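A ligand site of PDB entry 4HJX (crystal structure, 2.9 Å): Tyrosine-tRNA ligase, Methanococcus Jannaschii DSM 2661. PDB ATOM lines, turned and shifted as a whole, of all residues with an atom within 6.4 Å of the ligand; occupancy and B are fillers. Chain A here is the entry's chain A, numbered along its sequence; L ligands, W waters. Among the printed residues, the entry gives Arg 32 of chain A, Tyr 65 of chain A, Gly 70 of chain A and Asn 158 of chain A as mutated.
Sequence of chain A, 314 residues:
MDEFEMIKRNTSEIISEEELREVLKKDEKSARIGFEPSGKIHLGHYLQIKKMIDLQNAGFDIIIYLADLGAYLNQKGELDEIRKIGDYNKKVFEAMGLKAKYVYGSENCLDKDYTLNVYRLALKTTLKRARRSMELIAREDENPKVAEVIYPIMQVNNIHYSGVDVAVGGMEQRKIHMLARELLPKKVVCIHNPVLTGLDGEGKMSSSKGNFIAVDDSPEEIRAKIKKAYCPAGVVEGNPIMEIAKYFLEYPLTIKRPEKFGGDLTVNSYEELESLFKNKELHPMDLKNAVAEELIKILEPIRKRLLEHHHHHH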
ATOM      1  N   ARG A  32     -18.912 -25.952  -5.363  1.00  0.00           N
ATOM      2  CA  ARG A  32     -19.164 -27.234  -4.709  1.00  0.00           C
ATOM      3  C   ARG A  32     -20.391 -27.218  -3.804  1.00  0.00           C
ATOM      4  O   ARG A  32     -20.578 -26.316  -2.994  1.00  0.00           O
ATOM      5  CB  ARG A  32     -17.928 -27.661  -3.910  1.00  0.00           C
ATOM      6  CG  ARG A  32     -18.109 -28.923  -3.078  1.00  0.00           C
ATOM      7  CD  ARG A  32     -16.842 -29.218  -2.289  1.00  0.00           C
ATOM      8  NE  ARG A  32     -17.051 -30.242  -1.269  1.00  0.00           N
ATOM      9  CZ  ARG A  32     -17.431 -29.989  -0.030  1.00  0.00           C
ATOM     10  NH1 ARG A  32     -17.632 -28.742   0.364  1.00  0.00           N
ATOM     11  NH2 ARG A  32     -17.603 -30.991   0.831  1.00  0.00           N
ATOM     12  N   ILE A  33     -21.228 -28.241  -3.965  1.00  0.00           N
ATOM     13  CA  ILE A  33     -22.390 -28.424  -3.102  1.00  0.00           C
ATOM     14  C   ILE A  33     -22.398 -29.845  -2.530  1.00  0.00           C
ATOM     15  O   ILE A  33     -22.001 -30.801  -3.198  1.00  0.00           O
ATOM     16  CB  ILE A  33     -23.710 -28.139  -3.857  1.00  0.00           C
ATOM     17  CG1 ILE A  33     -24.907 -28.210  -2.906  1.00  0.00           C
ATOM     18  CG2 ILE A  33     -23.890 -29.093  -5.029  1.00  0.00           C
ATOM     19  CD1 ILE A  33     -26.196 -27.737  -3.522  1.00  0.00           C
ATOM     20  N   GLY A  34     -22.833 -29.977  -1.293  1.00  0.00           N
ATOM     21  CA  GLY A  34     -22.877 -31.265  -0.638  1.00  0.00           C
ATOM     22  C   GLY A  34     -24.275 -31.681  -0.229  1.00  0.00           C
ATOM     23  O   GLY A  34     -25.053 -30.864   0.271  1.00  0.00           O
ATOM     24  N   PHE A  35     -24.607 -32.958  -0.441  1.00  0.00           N
ATOM     25  CA  PHE A  35     -25.905 -33.483  -0.071  1.00  0.00           C
ATOM     26  C   PHE A  35     -25.758 -34.677   0.878  1.00  0.00           C
ATOM     27  O   PHE A  35     -24.898 -35.528   0.675  1.00  0.00           O
ATOM     28  CB  PHE A  35     -26.679 -33.944  -1.309  1.00  0.00           C
ATOM     29  CG  PHE A  35     -27.120 -32.822  -2.207  1.00  0.00           C
ATOM     30  CD1 PHE A  35     -26.455 -32.581  -3.389  1.00  0.00           C
ATOM     31  CD2 PHE A  35     -28.202 -32.030  -1.869  1.00  0.00           C
ATOM     32  CE1 PHE A  35     -26.861 -31.556  -4.226  1.00  0.00           C
ATOM     33  CE2 PHE A  35     -28.614 -31.007  -2.699  1.00  0.00           C
ATOM     34  CZ  PHE A  35     -27.938 -30.773  -3.874  1.00  0.00           C
ATOM     35  N   GLU A  36     -26.606 -34.724   1.894  1.00  0.00           N
ATOM     36  CA  GLU A  36     -26.785 -35.951   2.661  1.00  0.00           C
ATOM     37  C   GLU A  36     -27.636 -36.876   1.820  1.00  0.00           C
ATOM     38  O   GLU A  36     -28.748 -36.505   1.435  1.00  0.00           O
ATOM     39  CB  GLU A  36     -27.466 -35.678   4.002  1.00  0.00           C
ATOM     40  CG  GLU A  36     -26.657 -34.828   4.968  1.00  0.00           C
ATOM     41  CD  GLU A  36     -27.235 -34.829   6.362  1.00  0.00           C
ATOM     42  OE1 GLU A  36     -27.973 -35.782   6.704  1.00  0.00           O
ATOM     43  OE2 GLU A  36     -26.958 -33.875   7.126  1.00  0.00           O
ATOM     44  N   TYR A  65     -20.622 -33.177  -3.684  1.00  0.00           N
ATOM     45  CA  TYR A  65     -20.152 -33.913  -2.518  1.00  0.00           C
ATOM     46  C   TYR A  65     -21.276 -34.746  -1.910  1.00  0.00           C
ATOM     47  O   TYR A  65     -22.287 -34.210  -1.473  1.00  0.00           O
ATOM     48  CB  TYR A  65     -19.583 -32.955  -1.478  1.00  0.00           C
ATOM     49  CG  TYR A  65     -18.955 -33.620  -0.285  1.00  0.00           C
ATOM     50  CD1 TYR A  65     -19.622 -33.670   0.933  1.00  0.00           C
ATOM     51  CD2 TYR A  65     -17.695 -34.194  -0.363  1.00  0.00           C
ATOM     52  CE1 TYR A  65     -19.057 -34.292   2.040  1.00  0.00           C
ATOM     53  CE2 TYR A  65     -17.119 -34.811   0.729  1.00  0.00           C
ATOM     54  CZ  TYR A  65     -17.798 -34.854   1.927  1.00  0.00           C
ATOM     55  OH  TYR A  65     -17.231 -35.464   3.026  1.00  0.00           O
ATOM     56  N   ALA A  67     -22.251 -36.393   1.090  1.00  0.00           N
ATOM     57  CA  ALA A  67     -21.906 -36.448   2.505  1.00  0.00           C
ATOM     58  C   ALA A  67     -22.504 -37.650   3.208  1.00  0.00           C
ATOM     59  O   ALA A  67     -23.504 -37.539   3.927  1.00  0.00           O
ATOM     60  CB  ALA A  67     -22.331 -35.160   3.197  1.00  0.00           C
ATOM     61  N   GLY A  70     -21.516 -37.306   6.912  1.00  0.00           N
ATOM     62  CA  GLY A  70     -22.368 -36.308   7.533  1.00  0.00           C
ATOM     63  C   GLY A  70     -23.689 -36.898   7.955  1.00  0.00           C
ATOM     64  O   GLY A  70     -24.146 -36.692   9.082  1.00  0.00           O
ATOM     65  N   ASN A  74     -25.312 -37.574  11.527  1.00  0.00           N
ATOM     66  CA  ASN A  74     -26.627 -36.974  11.767  1.00  0.00           C
ATOM     67  C   ASN A  74     -27.685 -38.037  12.062  1.00  0.00           C
ATOM     68  O   ASN A  74     -28.882 -37.786  11.963  1.00  0.00           O
ATOM     69  CB  ASN A  74     -27.053 -36.124  10.569  1.00  0.00           C
ATOM     70  CG  ASN A  74     -27.998 -35.003  10.965  1.00  0.00           C
ATOM     71  OD1 ASN A  74     -28.570 -35.000  12.053  1.00  0.00           O
ATOM     72  ND2 ASN A  74     -28.173 -34.036  10.076  1.00  0.00           N
ATOM     73  N   ILE A 137     -30.507 -28.173  10.454  1.00  0.00           N
ATOM     74  CA  ILE A 137     -29.888 -29.323   9.799  1.00  0.00           C
ATOM     75  C   ILE A 137     -29.978 -30.604  10.629  1.00  0.00           C
ATOM     76  O   ILE A 137     -30.366 -31.654  10.125  1.00  0.00           O
ATOM     77  CB  ILE A 137     -28.403 -29.038   9.452  1.00  0.00           C
ATOM     78  CG1 ILE A 137     -28.296 -27.822   8.535  1.00  0.00           C
ATOM     79  CG2 ILE A 137     -27.768 -30.268   8.809  1.00  0.00           C
ATOM     80  CD1 ILE A 137     -26.874 -27.484   8.145  1.00  0.00           C
ATOM     81  N   TYR A 151     -20.240 -32.473  13.144  1.00  0.00           N
ATOM     82  CA  TYR A 151     -20.815 -32.253  11.816  1.00  0.00           C
ATOM     83  C   TYR A 151     -20.429 -30.899  11.184  1.00  0.00           C
ATOM     84  O   TYR A 151     -19.898 -30.884  10.072  1.00  0.00           O
ATOM     85  CB  TYR A 151     -22.340 -32.413  11.876  1.00  0.00           C
ATOM     86  CG  TYR A 151     -23.059 -32.431  10.541  1.00  0.00           C
ATOM     87  CD1 TYR A 151     -23.549 -33.617  10.018  1.00  0.00           C
ATOM     88  CD2 TYR A 151     -23.266 -31.259   9.826  1.00  0.00           C
ATOM     89  CE1 TYR A 151     -24.213 -33.629   8.806  1.00  0.00           C
ATOM     90  CE2 TYR A 151     -23.930 -31.271   8.614  1.00  0.00           C
ATOM     91  CZ  TYR A 151     -24.395 -32.458   8.110  1.00  0.00           C
ATOM     92  OH  TYR A 151     -25.065 -32.473   6.905  1.00  0.00           O
ATOM     93  N   MET A 154     -16.676 -30.236  10.376  1.00  0.00           N
ATOM     94  CA  MET A 154     -16.197 -31.079   9.288  1.00  0.00           C
ATOM     95  C   MET A 154     -16.591 -30.489   7.937  1.00  0.00           C
ATOM     96  O   MET A 154     -15.824 -30.551   6.978  1.00  0.00           O
ATOM     97  CB  MET A 154     -16.739 -32.494   9.417  1.00  0.00           C
ATOM     98  CG  MET A 154     -15.902 -33.399  10.311  1.00  0.00           C
ATOM     99  SD  MET A 154     -16.584 -35.070  10.403  1.00  0.00           S
ATOM    100  CE  MET A 154     -16.837 -35.429   8.672  1.00  0.00           C
ATOM    101  N   GLN A 155     -17.796 -29.932   7.881  1.00  0.00           N
ATOM    102  CA  GLN A 155     -18.272 -29.292   6.666  1.00  0.00           C
ATOM    103  C   GLN A 155     -17.416 -28.070   6.335  1.00  0.00           C
ATOM    104  O   GLN A 155     -17.139 -27.786   5.171  1.00  0.00           O
ATOM    105  CB  GLN A 155     -19.747 -28.890   6.808  1.00  0.00           C
ATOM    106  CG  GLN A 155     -20.322 -28.192   5.588  1.00  0.00           C
ATOM    107  CD  GLN A 155     -21.834 -28.257   5.534  1.00  0.00           C
ATOM    108  OE1 GLN A 155     -22.451 -29.008   6.283  1.00  0.00           O
ATOM    109  NE2 GLN A 155     -22.432 -27.474   4.651  1.00  0.00           N
ATOM    110  N   VAL A 156     -16.994 -27.361   7.375  1.00  0.00           N
ATOM    111  CA  VAL A 156     -16.075 -26.239   7.215  1.00  0.00           C
ATOM    112  C   VAL A 156     -14.711 -26.747   6.757  1.00  0.00           C
ATOM    113  O   VAL A 156     -14.102 -26.196   5.844  1.00  0.00           O
ATOM    114  CB  VAL A 156     -15.901 -25.466   8.543  1.00  0.00           C
ATOM    115  CG1 VAL A 156     -14.782 -24.452   8.433  1.00  0.00           C
ATOM    116  CG2 VAL A 156     -17.200 -24.791   8.923  1.00  0.00           C
ATOM    117  N   ASN A 158     -14.094 -29.467   5.159  1.00  0.00           N
ATOM    118  CA  ASN A 158     -14.232 -29.989   3.800  1.00  0.00           C
ATOM    119  C   ASN A 158     -14.169 -28.870   2.752  1.00  0.00           C
ATOM    120  O   ASN A 158     -13.608 -29.060   1.672  1.00  0.00           O
ATOM    121  CB  ASN A 158     -15.517 -30.799   3.642  1.00  0.00           C
ATOM    122  CG  ASN A 158     -15.436 -32.147   4.320  1.00  0.00           C
ATOM    123  OD1 ASN A 158     -14.349 -32.661   4.586  1.00  0.00           O
ATOM    124  ND2 ASN A 158     -16.594 -32.743   4.605  1.00  0.00           N
ATOM    125  N   ILE A 159     -14.756 -27.727   3.077  1.00  0.00           N
ATOM    126  CA  ILE A 159     -14.717 -26.561   2.210  1.00  0.00           C
ATOM    127  C   ILE A 159     -13.273 -26.105   2.031  1.00  0.00           C
ATOM    128  O   ILE A 159     -12.854 -25.717   0.945  1.00  0.00           O
ATOM    129  CB  ILE A 159     -15.574 -25.412   2.761  1.00  0.00           C
ATOM    130  CG1 ILE A 159     -17.064 -25.768   2.703  1.00  0.00           C
ATOM    131  CG2 ILE A 159     -15.328 -24.127   1.972  1.00  0.00           C
ATOM    132  CD1 ILE A 159     -17.967 -24.656   3.180  1.00  0.00           C
ATOM    133  N   VAL A 168     -22.150 -23.750  -2.410  1.00  0.00           N
ATOM    134  CA  VAL A 168     -23.586 -23.669  -2.670  1.00  0.00           C
ATOM    135  C   VAL A 168     -24.356 -24.584  -1.729  1.00  0.00           C
ATOM    136  O   VAL A 168     -23.881 -25.650  -1.346  1.00  0.00           O
ATOM    137  CB  VAL A 168     -23.900 -24.040  -4.139  1.00  0.00           C
ATOM    138  CG1 VAL A 168     -25.373 -23.822  -4.460  1.00  0.00           C
ATOM    139  CG2 VAL A 168     -23.027 -23.236  -5.092  1.00  0.00           C
ATOM    140  N   GLU A 172     -30.456 -23.294   4.970  1.00  0.00           N
ATOM    141  CA  GLU A 172     -30.213 -23.992   6.223  1.00  0.00           C
ATOM    142  C   GLU A 172     -28.712 -24.165   6.463  1.00  0.00           C
ATOM    143  O   GLU A 172     -28.286 -24.508   7.570  1.00  0.00           O
ATOM    144  CB  GLU A 172     -30.893 -25.358   6.223  1.00  0.00           C
ATOM    145  CG  GLU A 172     -32.292 -25.379   5.631  1.00  0.00           C
ATOM    146  CD  GLU A 172     -32.307 -25.753   4.168  1.00  0.00           C
ATOM    147  OE1 GLU A 172     -31.231 -25.742   3.534  1.00  0.00           O
ATOM    148  OE2 GLU A 172     -33.403 -26.067   3.644  1.00  0.00           O
ATOM    149  N   GLN A 173     -27.921 -23.935   5.425  1.00  0.00           N
ATOM    150  CA  GLN A 173     -26.481 -24.156   5.486  1.00  0.00           C
ATOM    151  C   GLN A 173     -25.706 -22.871   5.738  1.00  0.00           C
ATOM    152  O   GLN A 173     -24.482 -22.886   5.807  1.00  0.00           O
ATOM    153  CB  GLN A 173     -26.003 -24.797   4.178  1.00  0.00           C
ATOM    154  CG  GLN A 173     -26.798 -26.018   3.750  1.00  0.00           C
ATOM    155  CD  GLN A 173     -26.588 -27.208   4.656  1.00  0.00           C
ATOM    156  OE1 GLN A 173     -25.495 -27.420   5.171  1.00  0.00           O
ATOM    157  NE2 GLN A 173     -27.641 -27.996   4.852  1.00  0.00           N
ATOM    158  N   ILE A 176     -23.319 -22.432   9.018  1.00  0.00           N
ATOM    159  CA  ILE A 176     -22.093 -23.209   8.886  1.00  0.00           C
ATOM    160  C   ILE A 176     -21.135 -22.511   7.910  1.00  0.00           C
ATOM    161  O   ILE A 176     -19.936 -22.414   8.167  1.00  0.00           O
ATOM    162  CB  ILE A 176     -22.378 -24.639   8.399  1.00  0.00           C
ATOM    163  CG1 ILE A 176     -23.206 -25.397   9.439  1.00  0.00           C
ATOM    164  CG2 ILE A 176     -21.080 -25.383   8.124  1.00  0.00           C
ATOM    165  CD1 ILE A 176     -23.410 -26.856   9.121  1.00  0.00           C
ATOM    166  N   HIS A 177     -21.689 -22.014   6.809  1.00  0.00           N
ATOM    167  CA  HIS A 177     -20.904 -21.358   5.780  1.00  0.00           C
ATOM    168  C   HIS A 177     -20.301 -20.041   6.263  1.00  0.00           C
ATOM    169  O   HIS A 177     -19.172 -19.700   5.924  1.00  0.00           O
ATOM    170  CB  HIS A 177     -21.734 -21.132   4.521  1.00  0.00           C
ATOM    171  CG  HIS A 177     -21.986 -22.386   3.739  1.00  0.00           C
ATOM    172  ND1 HIS A 177     -22.780 -22.431   2.625  1.00  0.00           N
ATOM    173  CD2 HIS A 177     -21.528 -23.655   3.924  1.00  0.00           C
ATOM    174  CE1 HIS A 177     -22.815 -23.658   2.149  1.00  0.00           C
ATOM    175  NE2 HIS A 177     -22.061 -24.419   2.924  1.00  0.00           N
HETATM  176  O1  LIG L   1     -27.060 -31.898   3.482  1.00  0.00           O
HETATM  177  C1  LIG L   1     -26.636 -31.039   4.288  1.00  0.00           C
HETATM  178  O2  LIG L   1     -27.314 -30.446   5.153  1.00  0.00           O
HETATM  179  C2  LIG L   1     -25.157 -30.658   4.176  1.00  0.00           C
HETATM  180  N1  LIG L   1     -24.721 -30.028   5.434  1.00  0.00           N
HETATM  181  C3  LIG L   1     -24.338 -31.918   3.884  1.00  0.00           C
HETATM  182  C4  LIG L   1     -22.987 -31.598   3.785  1.00  0.00           C
HETATM  183  C5  LIG L   1     -22.089 -32.054   4.746  1.00  0.00           C
HETATM  184  C6  LIG L   1     -20.730 -31.740   4.624  1.00  0.00           C
HETATM  185  F1  LIG L   1     -19.840 -32.166   5.550  1.00  0.00           F
HETATM  186  C7  LIG L   1     -22.551 -30.839   2.706  1.00  0.00           C
HETATM  187  C8  LIG L   1     -21.202 -30.518   2.579  1.00  0.00           C
HETATM  188  F2  LIG L   1     -20.764 -29.780   1.521  1.00  0.00           F
HETATM  189  C9  LIG L   1     -20.318 -30.979   3.540  1.00  0.00           C
HETATM  190  O3  LIG L   1     -19.005 -30.662   3.424  1.00  0.00           O
HETATM  191  O   HOH W   1     -25.440 -28.527   1.616  1.00  0.00           O
HETATM  192  O   HOH W   2     -23.211 -27.656   0.237  1.00  0.00           O
HETATM  193  O   HOH W   3     -29.631 -30.704   1.519  1.00  0.00           O
HETATM  194  O   HOH W   4     -20.797 -26.494   1.853  1.00  0.00           O
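NE2 of Gln 173 lies within hydrogen-bond range of O2 of the ligand (2.5 Å). N1 of the ligand is in hydrogen-bond range of OE1 of Gln 155, 2.6 Å away. OH of Tyr 151 lies within hydrogen-bond range of N1 of the ligand, at 2.9 Å. NH2 of Arg 32 lies within hydrogen-bond range of O3 of the ligand (3.0 Å). An oxygen (O1) of the ligand lies within hydrogen-bond range of the backbone NH (N) of Glu 36. ND2 of Asn 158 is in hydrogen-bond range of O3 of the ligand, 3.4 Å away.
NE2 of Gln 155 sits at hydrogen-bond distance from OE1 of Gln 173 (3.1 Å). O of Arg 32 is in hydrogen-bond range of N of Val 168, 3.1 Å away. The side-chain carboxylate of Glu 36 is in hydrogen-bond range of the side-chain amide nitrogen of Asn 74. The side-chain amide nitrogen of Asn 158 lies close to the backbone carbonyl oxygen of Met 154, at 3.3 Å. The backbone NH of Ala 67 sits at hydrogen-bond distance from the backbone carbonyl oxygen of Phe 35 (2.8 Å). O of Ile 137 is in hydrogen-bond range of ND2 of Asn 74 (3.2 Å). The backbone NH (N) of Phe 35 lies within hydrogen-bond range of the backbone carbonyl oxygen (O) of Tyr 65 (2.8 Å). N of Tyr 65 lies within hydrogen-bond range of O of Ile 33.
F2 of the ligand lies close to N of Gly 34 (3.5 Å). CD1 of Tyr 65 touches C9 of the ligand, 3.8 Å away. CB of Ala 67 touches C5 of the ligand (3.5 Å). Ile 137 touches the ligand (CG2 to O2, 3.7 Å). Hydrophobic or aromatic side chains within 4 Å of the ligand: Tyr 65, Ala 67, Ile 137 and Tyr 151. The nearest printed residue that does not touch the ligand is Phe 35 (4.02 Å).
Water W4 lies within hydrogen-bond range of NE2 of His 177 (2.7 Å) and NE2 of Gln 155 (3.4 Å). Water W2 lies within hydrogen-bond range of O of Val 168 (2.6 Å) and N of Gly 34 (2.8 Å).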
